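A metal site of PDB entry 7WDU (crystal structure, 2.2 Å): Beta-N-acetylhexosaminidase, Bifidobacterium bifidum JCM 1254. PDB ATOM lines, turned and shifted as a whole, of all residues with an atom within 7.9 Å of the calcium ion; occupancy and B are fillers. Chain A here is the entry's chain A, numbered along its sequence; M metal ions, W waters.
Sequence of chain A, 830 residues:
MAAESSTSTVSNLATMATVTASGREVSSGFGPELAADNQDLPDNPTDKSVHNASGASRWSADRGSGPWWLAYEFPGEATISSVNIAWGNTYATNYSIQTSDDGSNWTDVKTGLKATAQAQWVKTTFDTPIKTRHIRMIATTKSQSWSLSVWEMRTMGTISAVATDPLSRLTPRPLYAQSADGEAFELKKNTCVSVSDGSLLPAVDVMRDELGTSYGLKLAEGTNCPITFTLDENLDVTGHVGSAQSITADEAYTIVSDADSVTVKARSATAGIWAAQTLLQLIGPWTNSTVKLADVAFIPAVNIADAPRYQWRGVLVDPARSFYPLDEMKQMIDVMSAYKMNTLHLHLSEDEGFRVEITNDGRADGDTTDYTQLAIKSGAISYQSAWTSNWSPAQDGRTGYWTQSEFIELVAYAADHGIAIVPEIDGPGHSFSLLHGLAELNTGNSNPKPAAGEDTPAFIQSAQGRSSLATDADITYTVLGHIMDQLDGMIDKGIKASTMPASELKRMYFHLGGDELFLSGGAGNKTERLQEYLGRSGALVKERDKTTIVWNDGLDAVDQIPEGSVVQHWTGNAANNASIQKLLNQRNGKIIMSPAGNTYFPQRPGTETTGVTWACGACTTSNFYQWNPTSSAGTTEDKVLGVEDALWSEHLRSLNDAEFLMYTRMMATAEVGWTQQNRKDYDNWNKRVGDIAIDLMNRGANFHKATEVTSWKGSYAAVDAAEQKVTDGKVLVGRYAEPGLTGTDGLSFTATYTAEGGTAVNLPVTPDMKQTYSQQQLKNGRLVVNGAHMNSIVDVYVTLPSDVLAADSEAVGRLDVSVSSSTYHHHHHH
The side-chain carboxylate (OD2) of Asp 37 lies within hydrogen-bond range of the side-chain amide nitrogen (NE2) of Gln 39, at 3.1 Å.
The backbone carbonyl oxygen of Ala 86 is in hydrogen-bond range of the backbone NH of Trp 151.
OE2 of Glu 152 lies close to N of Asn 38 (3.4 Å).
The backbone NH (N) of Gln 39 sits close to the side-chain carboxylate (OE1) of Glu 152, at 3.4 Å.
The guanidinium group of Arg 154 is in salt-bridge range of the side-chain carboxylate of Glu 152 (2.7 Å).
The backbone carbonyl oxygen of Glu 152 lies within hydrogen-bond range of the backbone NH of Ala 86, 2.9 Å away.
Of the 23 residues printed, 5 come within 4 Å of the calcium ion.
The calcium ion is bound by the backbone carbonyl oxygen (O) of Ser 57 (2.2 Å), the backbone carbonyl oxygen (O) of Trp 151 (2.4 Å), the backbone carbonyl oxygen (O) of Leu 34 (2.4 Å), the side-chain hydroxyl (OG) of Ser 57 (2.4 Å), water W1 (2.4 Å), the side-chain carboxylate (OE2) of Glu 152 (2.6 Å) and the side-chain carboxylate (OD1) of Asp 37 (2.7 Å).
The calcium ion has seven donor atoms within binding distance.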
ATOM      1  N   GLY A  31      16.618 -18.268  -7.318  1.00  0.00           N
ATOM      2  CA  GLY A  31      16.496 -18.015  -8.774  1.00  0.00           C
ATOM      3  C   GLY A  31      16.239 -19.306  -9.550  1.00  0.00           C
ATOM      4  O   GLY A  31      16.584 -20.403  -9.099  1.00  0.00           O
ATOM      5  N   PRO A  32      15.601 -19.191 -10.726  1.00  0.00           N
ATOM      6  CA  PRO A  32      15.303 -20.342 -11.566  1.00  0.00           C
ATOM      7  C   PRO A  32      16.534 -21.204 -11.825  1.00  0.00           C
ATOM      8  O   PRO A  32      16.376 -22.389 -11.876  1.00  0.00           O
ATOM      9  CB  PRO A  32      14.830 -19.773 -12.909  1.00  0.00           C
ATOM     10  CG  PRO A  32      14.731 -18.255 -12.733  1.00  0.00           C
ATOM     11  CD  PRO A  32      15.175 -17.915 -11.332  1.00  0.00           C
ATOM     12  N   GLU A  33      17.714 -20.600 -11.967  1.00  0.00           N
ATOM     13  CA  GLU A  33      18.951 -21.316 -12.345  1.00  0.00           C
ATOM     14  C   GLU A  33      19.293 -22.348 -11.259  1.00  0.00           C
ATOM     15  O   GLU A  33      20.016 -23.295 -11.589  1.00  0.00           O
ATOM     16  CB  GLU A  33      20.117 -20.347 -12.636  1.00  0.00           C
ATOM     17  CG  GLU A  33      20.731 -19.712 -11.384  1.00  0.00           C
ATOM     18  CD  GLU A  33      19.958 -18.527 -10.815  1.00  0.00           C
ATOM     19  OE1 GLU A  33      18.844 -18.209 -11.342  1.00  0.00           O
ATOM     20  OE2 GLU A  33      20.465 -17.928  -9.852  1.00  0.00           O
ATOM     21  N   LEU A  34      18.764 -22.187 -10.041  1.00  0.00           N
ATOM     22  CA  LEU A  34      19.072 -23.092  -8.900  1.00  0.00           C
ATOM     23  C   LEU A  34      18.279 -24.410  -9.020  1.00  0.00           C
ATOM     24  O   LEU A  34      18.630 -25.343  -8.305  1.00  0.00           O
ATOM     25  CB  LEU A  34      18.795 -22.360  -7.577  1.00  0.00           C
ATOM     26  CG  LEU A  34      19.698 -21.159  -7.296  1.00  0.00           C
ATOM     27  CD1 LEU A  34      19.344 -20.493  -5.965  1.00  0.00           C
ATOM     28  CD2 LEU A  34      21.185 -21.534  -7.300  1.00  0.00           C
ATOM     29  N   ALA A  35      17.326 -24.514  -9.935  1.00  0.00           N
ATOM     30  CA  ALA A  35      16.707 -25.803 -10.367  1.00  0.00           C
ATOM     31  C   ALA A  35      17.661 -26.575 -11.289  1.00  0.00           C
ATOM     32  O   ALA A  35      17.464 -27.777 -11.463  1.00  0.00           O
ATOM     33  CB  ALA A  35      15.396 -25.509 -11.050  1.00  0.00           C
ATOM     34  N   ALA A  36      18.646 -25.889 -11.885  1.00  0.00           N
ATOM     35  CA  ALA A  36      19.500 -26.401 -12.979  1.00  0.00           C
ATOM     36  C   ALA A  36      20.942 -26.659 -12.525  1.00  0.00           C
ATOM     37  O   ALA A  36      21.788 -26.874 -13.411  1.00  0.00           O
ATOM     38  CB  ALA A  36      19.498 -25.406 -14.120  1.00  0.00           C
ATOM     39  N   ASP A  37      21.235 -26.662 -11.226  1.00  0.00           N
ATOM     40  CA  ASP A  37      22.630 -26.810 -10.738  1.00  0.00           C
ATOM     41  C   ASP A  37      22.936 -28.271 -10.337  1.00  0.00           C
ATOM     42  O   ASP A  37      24.031 -28.487  -9.742  1.00  0.00           O
ATOM     43  CB  ASP A  37      22.946 -25.845  -9.582  1.00  0.00           C
ATOM     44  CG  ASP A  37      22.071 -26.082  -8.368  1.00  0.00           C
ATOM     45  OD1 ASP A  37      21.290 -27.064  -8.420  1.00  0.00           O
ATOM     46  OD2 ASP A  37      22.143 -25.268  -7.412  1.00  0.00           O
ATOM     47  N   ASN A  38      22.032 -29.220 -10.639  1.00  0.00           N
ATOM     48  CA  ASN A  38      22.286 -30.686 -10.516  1.00  0.00           C
ATOM     49  C   ASN A  38      22.746 -31.036  -9.091  1.00  0.00           C
ATOM     50  O   ASN A  38      23.672 -31.822  -8.908  1.00  0.00           O
ATOM     51  CB  ASN A  38      23.301 -31.144 -11.574  1.00  0.00           C
ATOM     52  CG  ASN A  38      23.446 -32.650 -11.684  1.00  0.00           C
ATOM     53  OD1 ASN A  38      22.460 -33.363 -11.868  1.00  0.00           O
ATOM     54  ND2 ASN A  38      24.683 -33.122 -11.623  1.00  0.00           N
ATOM     55  N   GLN A  39      22.157 -30.408  -8.081  1.00  0.00           N
ATOM     56  CA  GLN A  39      22.497 -30.654  -6.667  1.00  0.00           C
ATOM     57  C   GLN A  39      21.450 -31.581  -6.044  1.00  0.00           C
ATOM     58  O   GLN A  39      20.261 -31.275  -6.184  1.00  0.00           O
ATOM     59  CB  GLN A  39      22.510 -29.349  -5.877  1.00  0.00           C
ATOM     60  CG  GLN A  39      23.665 -28.441  -6.243  1.00  0.00           C
ATOM     61  CD  GLN A  39      23.879 -27.415  -5.150  1.00  0.00           C
ATOM     62  OE1 GLN A  39      23.569 -27.646  -3.975  1.00  0.00           O
ATOM     63  NE2 GLN A  39      24.414 -26.278  -5.529  1.00  0.00           N
ATOM     64  N   ASP A  40      21.910 -32.635  -5.367  1.00  0.00           N
ATOM     65  CA  ASP A  40      21.077 -33.587  -4.597  1.00  0.00           C
ATOM     66  C   ASP A  40      20.373 -32.821  -3.469  1.00  0.00           C
ATOM     67  O   ASP A  40      20.962 -31.839  -2.956  1.00  0.00           O
ATOM     68  CB  ASP A  40      21.936 -34.755  -4.098  1.00  0.00           C
ATOM     69  CG  ASP A  40      22.242 -35.754  -5.202  1.00  0.00           C
ATOM     70  OD1 ASP A  40      21.724 -35.586  -6.306  1.00  0.00           O
ATOM     71  OD2 ASP A  40      22.973 -36.709  -4.943  1.00  0.00           O
ATOM     72  N   LEU A  41      19.157 -33.226  -3.098  1.00  0.00           N
ATOM     73  CA  LEU A  41      18.406 -32.519  -2.018  1.00  0.00           C
ATOM     74  C   LEU A  41      19.284 -32.446  -0.775  1.00  0.00           C
ATOM     75  O   LEU A  41      20.024 -33.365  -0.457  1.00  0.00           O
ATOM     76  CB  LEU A  41      17.073 -33.215  -1.716  1.00  0.00           C
ATOM     77  CG  LEU A  41      15.824 -32.482  -2.209  1.00  0.00           C
ATOM     78  CD1 LEU A  41      15.988 -32.058  -3.668  1.00  0.00           C
ATOM     79  CD2 LEU A  41      14.594 -33.378  -2.057  1.00  0.00           C
ATOM     80  N   PRO A  42      19.276 -31.300  -0.051  1.00  0.00           N
ATOM     81  CA  PRO A  42      19.974 -31.215   1.237  1.00  0.00           C
ATOM     82  C   PRO A  42      19.374 -32.164   2.291  1.00  0.00           C
ATOM     83  O   PRO A  42      18.274 -32.641   2.088  1.00  0.00           O
ATOM     84  CB  PRO A  42      19.824 -29.747   1.649  1.00  0.00           C
ATOM     85  CG  PRO A  42      18.607 -29.259   0.867  1.00  0.00           C
ATOM     86  CD  PRO A  42      18.622 -30.047  -0.424  1.00  0.00           C
ATOM     87  N   ALA A  56      19.694 -21.693  -0.276  1.00  0.00           N
ATOM     88  CA  ALA A  56      19.088 -23.000  -0.646  1.00  0.00           C
ATOM     89  C   ALA A  56      19.007 -23.133  -2.179  1.00  0.00           C
ATOM     90  O   ALA A  56      18.547 -22.182  -2.855  1.00  0.00           O
ATOM     91  CB  ALA A  56      17.725 -23.153  -0.016  1.00  0.00           C
ATOM     92  N   SER A  57      19.428 -24.286  -2.707  1.00  0.00           N
ATOM     93  CA  SER A  57      19.607 -24.610  -4.144  1.00  0.00           C
ATOM     94  C   SER A  57      18.268 -24.986  -4.774  1.00  0.00           C
ATOM     95  O   SER A  57      18.126 -26.160  -5.178  1.00  0.00           O
ATOM     96  CB  SER A  57      20.610 -25.727  -4.333  1.00  0.00           C
ATOM     97  OG  SER A  57      20.733 -26.028  -5.707  1.00  0.00           O
ATOM     98  N   ARG A  58      17.333 -24.040  -4.798  1.00  0.00           N
ATOM     99  CA  ARG A  58      15.973 -24.225  -5.354  1.00  0.00           C
ATOM    100  C   ARG A  58      15.462 -22.937  -6.005  1.00  0.00           C
ATOM    101  O   ARG A  58      15.895 -21.819  -5.609  1.00  0.00           O
ATOM    102  CB  ARG A  58      15.004 -24.647  -4.246  1.00  0.00           C
ATOM    103  CG  ARG A  58      14.781 -23.588  -3.193  1.00  0.00           C
ATOM    104  CD  ARG A  58      13.853 -24.124  -2.126  1.00  0.00           C
ATOM    105  NE  ARG A  58      13.426 -23.094  -1.180  1.00  0.00           N
ATOM    106  CZ  ARG A  58      12.421 -22.237  -1.368  1.00  0.00           C
ATOM    107  NH1 ARG A  58      11.701 -22.273  -2.469  1.00  0.00           N
ATOM    108  NH2 ARG A  58      12.140 -21.355  -0.412  1.00  0.00           N
ATOM    109  N   TRP A  59      14.544 -23.101  -6.950  1.00  0.00           N
ATOM    110  CA  TRP A  59      13.730 -22.009  -7.493  1.00  0.00           C
ATOM    111  C   TRP A  59      12.557 -21.738  -6.543  1.00  0.00           C
ATOM    112  O   TRP A  59      11.840 -22.687  -6.216  1.00  0.00           O
ATOM    113  CB  TRP A  59      13.228 -22.393  -8.884  1.00  0.00           C
ATOM    114  CG  TRP A  59      12.309 -21.379  -9.514  1.00  0.00           C
ATOM    115  CD1 TRP A  59      12.501 -20.022  -9.572  1.00  0.00           C
ATOM    116  CD2 TRP A  59      11.101 -21.644 -10.239  1.00  0.00           C
ATOM    117  NE1 TRP A  59      11.490 -19.434 -10.278  1.00  0.00           N
ATOM    118  CE2 TRP A  59      10.616 -20.396 -10.693  1.00  0.00           C
ATOM    119  CE3 TRP A  59      10.394 -22.804 -10.547  1.00  0.00           C
ATOM    120  CZ2 TRP A  59       9.432 -20.281 -11.418  1.00  0.00           C
ATOM    121  CZ3 TRP A  59       9.221 -22.695 -11.264  1.00  0.00           C
ATOM    122  CH2 TRP A  59       8.753 -21.450 -11.690  1.00  0.00           C
ATOM    123  N   ALA A  86      12.325 -32.472  -8.481  1.00  0.00           N
ATOM    124  CA  ALA A  86      12.316 -32.479  -6.994  1.00  0.00           C
ATOM    125  C   ALA A  86      11.554 -31.226  -6.556  1.00  0.00           C
ATOM    126  O   ALA A  86      12.148 -30.125  -6.631  1.00  0.00           O
ATOM    127  CB  ALA A  86      13.704 -32.520  -6.422  1.00  0.00           C
ATOM    128  N   TRP A 121      10.580 -36.329  -5.587  1.00  0.00           N
ATOM    129  CA  TRP A 121      11.021 -36.543  -6.982  1.00  0.00           C
ATOM    130  C   TRP A 121       9.830 -37.083  -7.758  1.00  0.00           C
ATOM    131  O   TRP A 121       9.345 -38.125  -7.351  1.00  0.00           O
ATOM    132  CB  TRP A 121      12.218 -37.512  -7.064  1.00  0.00           C
ATOM    133  CG  TRP A 121      13.505 -36.906  -6.607  1.00  0.00           C
ATOM    134  CD1 TRP A 121      14.072 -37.017  -5.377  1.00  0.00           C
ATOM    135  CD2 TRP A 121      14.378 -36.057  -7.382  1.00  0.00           C
ATOM    136  NE1 TRP A 121      15.240 -36.323  -5.330  1.00  0.00           N
ATOM    137  CE2 TRP A 121      15.447 -35.714  -6.536  1.00  0.00           C
ATOM    138  CE3 TRP A 121      14.360 -35.568  -8.694  1.00  0.00           C
ATOM    139  CZ2 TRP A 121      16.500 -34.893  -6.960  1.00  0.00           C
ATOM    140  CZ3 TRP A 121      15.374 -34.736  -9.104  1.00  0.00           C
ATOM    141  CH2 TRP A 121      16.443 -34.439  -8.253  1.00  0.00           C
ATOM    142  N   VAL A 150      10.960 -25.478  -6.516  1.00  0.00           N
ATOM    143  CA  VAL A 150      11.618 -26.545  -7.336  1.00  0.00           C
ATOM    144  C   VAL A 150      13.083 -26.605  -6.925  1.00  0.00           C
ATOM    145  O   VAL A 150      13.841 -25.645  -7.223  1.00  0.00           O
ATOM    146  CB  VAL A 150      11.461 -26.297  -8.843  1.00  0.00           C
ATOM    147  CG1 VAL A 150      12.312 -27.246  -9.650  1.00  0.00           C
ATOM    148  CG2 VAL A 150      10.011 -26.424  -9.242  1.00  0.00           C
ATOM    149  N   TRP A 151      13.465 -27.669  -6.209  1.00  0.00           N
ATOM    150  CA  TRP A 151      14.875 -27.929  -5.861  1.00  0.00           C
ATOM    151  C   TRP A 151      15.636 -28.221  -7.172  1.00  0.00           C
ATOM    152  O   TRP A 151      16.796 -27.752  -7.351  1.00  0.00           O
ATOM    153  CB  TRP A 151      15.007 -29.098  -4.875  1.00  0.00           C
ATOM    154  CG  TRP A 151      14.553 -28.891  -3.467  1.00  0.00           C
ATOM    155  CD1 TRP A 151      13.440 -29.430  -2.895  1.00  0.00           C
ATOM    156  CD2 TRP A 151      15.227 -28.180  -2.414  1.00  0.00           C
ATOM    157  NE1 TRP A 151      13.368 -29.099  -1.560  1.00  0.00           N
ATOM    158  CE2 TRP A 151      14.441 -28.309  -1.248  1.00  0.00           C
ATOM    159  CE3 TRP A 151      16.420 -27.462  -2.343  1.00  0.00           C
ATOM    160  CZ2 TRP A 151      14.821 -27.745  -0.035  1.00  0.00           C
ATOM    161  CZ3 TRP A 151      16.781 -26.874  -1.151  1.00  0.00           C
ATOM    162  CH2 TRP A 151      15.987 -27.017  -0.014  1.00  0.00           C
ATOM    163  N   GLU A 152      15.028 -29.028  -8.038  1.00  0.00           N
ATOM    164  CA  GLU A 152      15.703 -29.601  -9.233  1.00  0.00           C
ATOM    165  C   GLU A 152      14.711 -29.891 -10.350  1.00  0.00           C
ATOM    166  O   GLU A 152      13.688 -30.528 -10.092  1.00  0.00           O
ATOM    167  CB  GLU A 152      16.386 -30.919  -8.869  1.00  0.00           C
ATOM    168  CG  GLU A 152      17.568 -30.745  -7.951  1.00  0.00           C
ATOM    169  CD  GLU A 152      18.849 -30.403  -8.686  1.00  0.00           C
ATOM    170  OE1 GLU A 152      19.209 -31.188  -9.556  1.00  0.00           O
ATOM    171  OE2 GLU A 152      19.483 -29.378  -8.346  1.00  0.00           O
ATOM    172  N   MET A 153      15.027 -29.461 -11.570  1.00  0.00           N
ATOM    173  CA  MET A 153      14.455 -30.073 -12.799  1.00  0.00           C
ATOM    174  C   MET A 153      15.607 -30.708 -13.558  1.00  0.00           C
ATOM    175  O   MET A 153      16.404 -29.978 -14.129  1.00  0.00           O
ATOM    176  CB  MET A 153      13.745 -29.070 -13.699  1.00  0.00           C
ATOM    177  CG  MET A 153      13.031 -29.742 -14.830  1.00  0.00           C
ATOM    178  SD  MET A 153      11.760 -28.661 -15.473  1.00  0.00           S
ATOM    179  CE  MET A 153      12.739 -27.385 -16.277  1.00  0.00           C
ATOM    180  N   ARG A 154      15.686 -32.039 -13.525  1.00  0.00           N
ATOM    181  CA  ARG A 154      16.734 -32.813 -14.238  1.00  0.00           C
ATOM    182  C   ARG A 154      16.155 -33.299 -15.567  1.00  0.00           C
ATOM    183  O   ARG A 154      15.175 -34.074 -15.556  1.00  0.00           O
ATOM    184  CB  ARG A 154      17.208 -33.948 -13.325  1.00  0.00           C
ATOM    185  CG  ARG A 154      17.735 -33.457 -11.984  1.00  0.00           C
ATOM    186  CD  ARG A 154      18.750 -34.394 -11.368  1.00  0.00           C
ATOM    187  NE  ARG A 154      19.293 -33.785 -10.169  1.00  0.00           N
ATOM    188  CZ  ARG A 154      20.086 -34.409  -9.301  1.00  0.00           C
ATOM    189  NH1 ARG A 154      20.404 -35.678  -9.499  1.00  0.00           N
ATOM    190  NH2 ARG A 154      20.536 -33.777  -8.238  1.00  0.00           N
HETATM  191 CA    CA M   1      19.057 -27.221  -6.918  1.00  0.00          CA
HETATM  192  O   HOH W   1      19.008 -29.215  -5.559  1.00  0.00           O
